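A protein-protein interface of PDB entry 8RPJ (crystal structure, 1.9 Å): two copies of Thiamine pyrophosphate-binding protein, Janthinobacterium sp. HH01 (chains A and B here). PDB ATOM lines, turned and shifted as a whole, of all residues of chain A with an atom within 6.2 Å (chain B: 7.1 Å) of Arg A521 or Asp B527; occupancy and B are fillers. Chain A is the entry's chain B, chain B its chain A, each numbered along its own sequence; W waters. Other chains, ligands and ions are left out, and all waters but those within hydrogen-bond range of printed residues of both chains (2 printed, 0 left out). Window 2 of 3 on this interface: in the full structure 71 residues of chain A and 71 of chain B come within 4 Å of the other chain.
NH2 of Arg A521 lies within hydrogen-bond range of O of Ala B524 (2.8 Å).
OD1 of Asp B527 is in salt-bridge range of NH2 of Arg A521 (2.8 Å).
O of Ala A524 sits at hydrogen-bond distance from NH2 of Arg B521 (2.7 Å).
The backbone NH of Arg A521 is in hydrogen-bond range of the side-chain carboxylate of Asp A518 (3.1 Å).
Among the printed residues, pairs that only touch across the chains: Leu A522 with Phe B526 (3.3 Å), Arg A521 with Ala B525 (3.4 Å), Leu A522 with Leu B522 (3.5 Å), Ala A525 with Arg B521 (3.5 Å), Leu A522 with Ala B525 (3.6 Å), Phe A526 with Leu B522 (3.6 Å) and Ala A525 with Leu B522 (3.8 Å).
Printed residues of chain B within 4 Å of Arg A521: Ala B524, Ala B525 and Asp B527.
Ala A523 touches none of the printed residues of chain B.
Printed residues of chain B within 4 Å of Ala A525: Arg B521 and Leu B522.
Of the printed residues of chain A, Phe B526 touches Leu A522 (3.3 Å).
Printed residues of chain A within 4 Å of Asp B527: Arg A521 (2.8 Å).
The nearest printed residue of chain A that does not touch Asp B527 is Asp A518 (6.9 Å).
Of the 12 printed residues of chain B, 6 touch a printed residue of chain A.
Among the printed residues, Asp or Glu carboxylates within 4 Å of a Lys or Arg side-chain nitrogen of the other chain: Arg A521 with Asp B527 (2.8 Å).
Arg A521 touches Ala B524, and with the chains exchanged Ala A524 touches Arg B521.
Arg A521 touches Ala B525, and with the chains exchanged Ala A525 touches Arg B521.
Leu A522 touches Ala B525, and with the chains exchanged Ala A525 touches Leu B522.
Leu A522 touches Phe B526, and with the chains exchanged Phe A526 touches Leu B522.
Positions printed for both chains: 521, 522, 523, 524, 525 and 526.
Water W1 bridges NE of Arg B521 and O of Ala A524.
Water W2 bridges the backbone carbonyl oxygen (O) of Ala B525 and the backbone NH (N) of Asp A518.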
ATOM      1  N   ASP A 518      23.997 -14.529  -2.300  1.00  0.00           N
ATOM      2  CA  ASP A 518      22.595 -14.633  -2.704  1.00  0.00           C
ATOM      3  C   ASP A 518      22.556 -15.561  -3.908  1.00  0.00           C
ATOM      4  O   ASP A 518      22.939 -15.178  -5.013  1.00  0.00           O
ATOM      5  CB  ASP A 518      22.049 -13.245  -3.022  1.00  0.00           C
ATOM      6  CG  ASP A 518      20.600 -13.251  -3.497  1.00  0.00           C
ATOM      7  OD1 ASP A 518      20.130 -14.250  -4.077  1.00  0.00           O
ATOM      8  OD2 ASP A 518      19.937 -12.211  -3.302  1.00  0.00           O
ATOM      9  N   PHE A 519      22.117 -16.801  -3.700  1.00  0.00           N
ATOM     10  CA  PHE A 519      22.228 -17.791  -4.765  1.00  0.00           C
ATOM     11  C   PHE A 519      21.265 -17.533  -5.909  1.00  0.00           C
ATOM     12  O   PHE A 519      21.507 -18.011  -7.020  1.00  0.00           O
ATOM     13  CB  PHE A 519      22.026 -19.188  -4.192  1.00  0.00           C
ATOM     14  CG  PHE A 519      23.134 -19.606  -3.278  1.00  0.00           C
ATOM     15  CD1 PHE A 519      24.349 -20.017  -3.797  1.00  0.00           C
ATOM     16  CD2 PHE A 519      22.977 -19.564  -1.906  1.00  0.00           C
ATOM     17  CE1 PHE A 519      25.379 -20.390  -2.962  1.00  0.00           C
ATOM     18  CE2 PHE A 519      24.005 -19.937  -1.071  1.00  0.00           C
ATOM     19  CZ  PHE A 519      25.209 -20.349  -1.598  1.00  0.00           C
ATOM     20  N   SER A 520      20.197 -16.775  -5.681  1.00  0.00           N
ATOM     21  CA  SER A 520      19.333 -16.405  -6.795  1.00  0.00           C
ATOM     22  C   SER A 520      20.014 -15.391  -7.703  1.00  0.00           C
ATOM     23  O   SER A 520      19.821 -15.422  -8.923  1.00  0.00           O
ATOM     24  CB  SER A 520      18.002 -15.871  -6.267  1.00  0.00           C
ATOM     25  OG  SER A 520      17.199 -16.932  -5.791  1.00  0.00           O
ATOM     26  N   ARG A 521      20.833 -14.503  -7.136  1.00  0.00           N
ATOM     27  CA  ARG A 521      21.594 -13.579  -7.966  1.00  0.00           C
ATOM     28  C   ARG A 521      22.722 -14.303  -8.689  1.00  0.00           C
ATOM     29  O   ARG A 521      23.003 -14.011  -9.856  1.00  0.00           O
ATOM     30  CB  ARG A 521      22.118 -12.436  -7.106  1.00  0.00           C
ATOM     31  CG  ARG A 521      20.991 -11.556  -6.606  1.00  0.00           C
ATOM     32  CD  ARG A 521      21.477 -10.544  -5.611  1.00  0.00           C
ATOM     33  NE  ARG A 521      22.481  -9.666  -6.194  1.00  0.00           N
ATOM     34  CZ  ARG A 521      23.225  -8.832  -5.487  1.00  0.00           C
ATOM     35  NH1 ARG A 521      23.113  -8.758  -4.171  1.00  0.00           N
ATOM     36  NH2 ARG A 521      24.104  -8.055  -6.111  1.00  0.00           N
ATOM     37  N   LEU A 522      23.366 -15.265  -8.025  1.00  0.00           N
ATOM     38  CA  LEU A 522      24.342 -16.085  -8.729  1.00  0.00           C
ATOM     39  C   LEU A 522      23.671 -16.889  -9.838  1.00  0.00           C
ATOM     40  O   LEU A 522      24.218 -17.021 -10.939  1.00  0.00           O
ATOM     41  CB  LEU A 522      25.053 -17.038  -7.777  1.00  0.00           C
ATOM     42  CG  LEU A 522      26.125 -16.501  -6.834  1.00  0.00           C
ATOM     43  CD1 LEU A 522      26.736 -17.674  -6.075  1.00  0.00           C
ATOM     44  CD2 LEU A 522      27.185 -15.742  -7.582  1.00  0.00           C
ATOM     45  N   ALA A 523      22.493 -17.454  -9.561  1.00  0.00           N
ATOM     46  CA  ALA A 523      21.782 -18.214 -10.582  1.00  0.00           C
ATOM     47  C   ALA A 523      21.594 -17.373 -11.838  1.00  0.00           C
ATOM     48  O   ALA A 523      21.875 -17.827 -12.951  1.00  0.00           O
ATOM     49  CB  ALA A 523      20.431 -18.697 -10.042  1.00  0.00           C
ATOM     50  N   ALA A 524      21.145 -16.126 -11.671  1.00  0.00           N
ATOM     51  CA  ALA A 524      20.961 -15.252 -12.823  1.00  0.00           C
ATOM     52  C   ALA A 524      22.277 -15.025 -13.563  1.00  0.00           C
ATOM     53  O   ALA A 524      22.303 -14.992 -14.798  1.00  0.00           O
ATOM     54  CB  ALA A 524      20.352 -13.922 -12.378  1.00  0.00           C
ATOM     55  N   ALA A 525      23.382 -14.881 -12.827  1.00  0.00           N
ATOM     56  CA  ALA A 525      24.675 -14.669 -13.474  1.00  0.00           C
ATOM     57  C   ALA A 525      25.077 -15.861 -14.339  1.00  0.00           C
ATOM     58  O   ALA A 525      25.754 -15.682 -15.360  1.00  0.00           O
ATOM     59  CB  ALA A 525      25.757 -14.399 -12.425  1.00  0.00           C
ATOM     60  N   PHE A 526      24.689 -17.077 -13.939  1.00  0.00           N
ATOM     61  CA  PHE A 526      24.975 -18.294 -14.688  1.00  0.00           C
ATOM     62  C   PHE A 526      23.890 -18.633 -15.712  1.00  0.00           C
ATOM     63  O   PHE A 526      23.975 -19.686 -16.356  1.00  0.00           O
ATOM     64  CB  PHE A 526      25.116 -19.505 -13.752  1.00  0.00           C
ATOM     65  CG  PHE A 526      26.450 -19.625 -13.072  1.00  0.00           C
ATOM     66  CD1 PHE A 526      27.545 -20.160 -13.731  1.00  0.00           C
ATOM     67  CD2 PHE A 526      26.597 -19.226 -11.755  1.00  0.00           C
ATOM     68  CE1 PHE A 526      28.766 -20.273 -13.089  1.00  0.00           C
ATOM     69  CE2 PHE A 526      27.813 -19.339 -11.115  1.00  0.00           C
ATOM     70  CZ  PHE A 526      28.896 -19.865 -11.782  1.00  0.00           C
ATOM     71  N   ALA A 530      15.740 -19.207 -11.304  1.00  0.00           N
ATOM     72  CA  ALA A 530      15.824 -19.276  -9.854  1.00  0.00           C
ATOM     73  C   ALA A 530      14.497 -18.900  -9.220  1.00  0.00           C
ATOM     74  O   ALA A 530      13.773 -18.037  -9.728  1.00  0.00           O
ATOM     75  CB  ALA A 530      16.921 -18.340  -9.312  1.00  0.00           C
ATOM     76  N   GLU A 556      15.989 -21.462  -3.700  1.00  0.00           N
ATOM     77  CA  GLU A 556      16.438 -21.197  -2.342  1.00  0.00           C
ATOM     78  C   GLU A 556      15.281 -21.372  -1.369  1.00  0.00           C
ATOM     79  O   GLU A 556      14.158 -20.931  -1.635  1.00  0.00           O
ATOM     80  CB  GLU A 556      16.986 -19.778  -2.215  1.00  0.00           C
ATOM     81  CG  GLU A 556      18.310 -19.517  -2.889  1.00  0.00           C
ATOM     82  CD  GLU A 556      18.728 -18.064  -2.738  1.00  0.00           C
ATOM     83  OE1 GLU A 556      18.088 -17.204  -3.376  1.00  0.00           O
ATOM     84  OE2 GLU A 556      19.666 -17.789  -1.964  1.00  0.00           O
ATOM     85  N   VAL B 474      34.644 -10.469  -0.532  1.00  0.00           N
ATOM     86  CA  VAL B 474      33.621  -9.458  -0.318  1.00  0.00           C
ATOM     87  C   VAL B 474      33.273  -9.379   1.161  1.00  0.00           C
ATOM     88  O   VAL B 474      33.044  -8.292   1.698  1.00  0.00           O
ATOM     89  CB  VAL B 474      32.382  -9.742  -1.177  1.00  0.00           C
ATOM     90  CG1 VAL B 474      31.300  -8.723  -0.889  1.00  0.00           C
ATOM     91  CG2 VAL B 474      32.749  -9.692  -2.637  1.00  0.00           C
ATOM     92  N   ASN B 477      35.759  -7.327   2.657  1.00  0.00           N
ATOM     93  CA  ASN B 477      35.943  -6.105   1.877  1.00  0.00           C
ATOM     94  C   ASN B 477      37.414  -5.898   1.504  1.00  0.00           C
ATOM     95  O   ASN B 477      37.962  -4.797   1.619  1.00  0.00           O
ATOM     96  CB  ASN B 477      35.398  -4.893   2.632  1.00  0.00           C
ATOM     97  CG  ASN B 477      35.134  -3.706   1.725  1.00  0.00           C
ATOM     98  OD1 ASN B 477      34.700  -3.871   0.584  1.00  0.00           O
ATOM     99  ND2 ASN B 477      35.404  -2.503   2.222  1.00  0.00           N
ATOM    100  N   ARG B 521      29.033 -10.483 -14.837  1.00  0.00           N
ATOM    101  CA  ARG B 521      27.734 -10.788 -14.246  1.00  0.00           C
ATOM    102  C   ARG B 521      27.904 -11.469 -12.895  1.00  0.00           C
ATOM    103  O   ARG B 521      27.164 -11.175 -11.948  1.00  0.00           O
ATOM    104  CB  ARG B 521      26.912 -11.645 -15.208  1.00  0.00           C
ATOM    105  CG  ARG B 521      26.430 -10.840 -16.392  1.00  0.00           C
ATOM    106  CD  ARG B 521      25.801 -11.703 -17.443  1.00  0.00           C
ATOM    107  NE  ARG B 521      24.578 -12.344 -16.978  1.00  0.00           N
ATOM    108  CZ  ARG B 521      23.969 -13.319 -17.632  1.00  0.00           C
ATOM    109  NH1 ARG B 521      24.451 -13.788 -18.770  1.00  0.00           N
ATOM    110  NH2 ARG B 521      22.858 -13.846 -17.127  1.00  0.00           N
ATOM    111  N   LEU B 522      28.887 -12.363 -12.780  1.00  0.00           N
ATOM    112  CA  LEU B 522      29.167 -13.009 -11.502  1.00  0.00           C
ATOM    113  C   LEU B 522      29.612 -11.989 -10.464  1.00  0.00           C
ATOM    114  O   LEU B 522      29.150 -12.022  -9.317  1.00  0.00           O
ATOM    115  CB  LEU B 522      30.229 -14.082 -11.712  1.00  0.00           C
ATOM    116  CG  LEU B 522      30.312 -15.290 -10.782  1.00  0.00           C
ATOM    117  CD1 LEU B 522      28.961 -15.936 -10.601  1.00  0.00           C
ATOM    118  CD2 LEU B 522      31.313 -16.296 -11.357  1.00  0.00           C
ATOM    119  N   ALA B 523      30.499 -11.072 -10.858  1.00  0.00           N
ATOM    120  CA  ALA B 523      30.908  -9.994  -9.972  1.00  0.00           C
ATOM    121  C   ALA B 523      29.701  -9.262  -9.398  1.00  0.00           C
ATOM    122  O   ALA B 523      29.610  -9.041  -8.186  1.00  0.00           O
ATOM    123  CB  ALA B 523      31.813  -9.018 -10.730  1.00  0.00           C
ATOM    124  N   ALA B 524      28.766  -8.864 -10.262  1.00  0.00           N
ATOM    125  CA  ALA B 524      27.585  -8.153  -9.785  1.00  0.00           C
ATOM    126  C   ALA B 524      26.807  -8.991  -8.777  1.00  0.00           C
ATOM    127  O   ALA B 524      26.316  -8.466  -7.773  1.00  0.00           O
ATOM    128  CB  ALA B 524      26.692  -7.765 -10.962  1.00  0.00           C
ATOM    129  N   ALA B 525      26.687 -10.296  -9.024  1.00  0.00           N
ATOM    130  CA  ALA B 525      25.943 -11.148  -8.101  1.00  0.00           C
ATOM    131  C   ALA B 525      26.586 -11.163  -6.719  1.00  0.00           C
ATOM    132  O   ALA B 525      25.882 -11.292  -5.709  1.00  0.00           O
ATOM    133  CB  ALA B 525      25.843 -12.571  -8.658  1.00  0.00           C
ATOM    134  N   PHE B 526      27.911 -11.024  -6.660  1.00  0.00           N
ATOM    135  CA  PHE B 526      28.665 -10.952  -5.415  1.00  0.00           C
ATOM    136  C   PHE B 526      28.794  -9.533  -4.870  1.00  0.00           C
ATOM    137  O   PHE B 526      29.506  -9.333  -3.878  1.00  0.00           O
ATOM    138  CB  PHE B 526      30.085 -11.510  -5.608  1.00  0.00           C
ATOM    139  CG  PHE B 526      30.171 -13.010  -5.572  1.00  0.00           C
ATOM    140  CD1 PHE B 526      30.201 -13.684  -4.362  1.00  0.00           C
ATOM    141  CD2 PHE B 526      30.252 -13.741  -6.745  1.00  0.00           C
ATOM    142  CE1 PHE B 526      30.285 -15.065  -4.320  1.00  0.00           C
ATOM    143  CE2 PHE B 526      30.345 -15.123  -6.713  1.00  0.00           C
ATOM    144  CZ  PHE B 526      30.355 -15.785  -5.501  1.00  0.00           C
ATOM    145  N   ASP B 527      28.161  -8.546  -5.510  1.00  0.00           N
ATOM    146  CA  ASP B 527      28.278  -7.134  -5.122  1.00  0.00           C
ATOM    147  C   ASP B 527      29.704  -6.602  -5.296  1.00  0.00           C
ATOM    148  O   ASP B 527      30.175  -5.764  -4.520  1.00  0.00           O
ATOM    149  CB  ASP B 527      27.807  -6.914  -3.677  1.00  0.00           C
ATOM    150  CG  ASP B 527      26.288  -6.938  -3.533  1.00  0.00           C
ATOM    151  OD1 ASP B 527      25.591  -6.376  -4.405  1.00  0.00           O
ATOM    152  OD2 ASP B 527      25.792  -7.521  -2.544  1.00  0.00           O
ATOM    153  N   ILE B 528      30.394  -7.067  -6.326  1.00  0.00           N
ATOM    154  CA  ILE B 528      31.742  -6.606  -6.665  1.00  0.00           C
ATOM    155  C   ILE B 528      31.647  -5.738  -7.912  1.00  0.00           C
ATOM    156  O   ILE B 528      31.079  -6.183  -8.916  1.00  0.00           O
ATOM    157  CB  ILE B 528      32.711  -7.784  -6.903  1.00  0.00           C
ATOM    158  CG1 ILE B 528      32.887  -8.631  -5.638  1.00  0.00           C
ATOM    159  CG2 ILE B 528      34.065  -7.275  -7.412  1.00  0.00           C
ATOM    160  CD1 ILE B 528      33.597  -9.977  -5.873  1.00  0.00           C
ATOM    161  N   PRO B 529      32.173  -4.509  -7.900  1.00  0.00           N
ATOM    162  CA  PRO B 529      32.189  -3.719  -9.142  1.00  0.00           C
ATOM    163  C   PRO B 529      33.040  -4.393 -10.212  1.00  0.00           C
ATOM    164  O   PRO B 529      34.076  -4.998  -9.917  1.00  0.00           O
ATOM    165  CB  PRO B 529      32.776  -2.367  -8.715  1.00  0.00           C
ATOM    166  CG  PRO B 529      33.419  -2.606  -7.394  1.00  0.00           C
ATOM    167  CD  PRO B 529      32.694  -3.751  -6.749  1.00  0.00           C
ATOM    168  N   PRO B 552      37.166  -4.600  -3.261  1.00  0.00           N
ATOM    169  CA  PRO B 552      37.442  -5.549  -4.344  1.00  0.00           C
ATOM    170  C   PRO B 552      36.872  -5.089  -5.675  1.00  0.00           C
ATOM    171  O   PRO B 552      35.821  -4.444  -5.746  1.00  0.00           O
ATOM    172  CB  PRO B 552      36.769  -6.847  -3.873  1.00  0.00           C
ATOM    173  CG  PRO B 552      35.762  -6.420  -2.855  1.00  0.00           C
ATOM    174  CD  PRO B 552      36.252  -5.145  -2.240  1.00  0.00           C
HETATM  175  O   HOH W   1      23.103 -11.754 -14.877  1.00  0.00           O
HETATM  176  O   HOH W   2      25.462 -12.138  -3.168  1.00  0.00           O
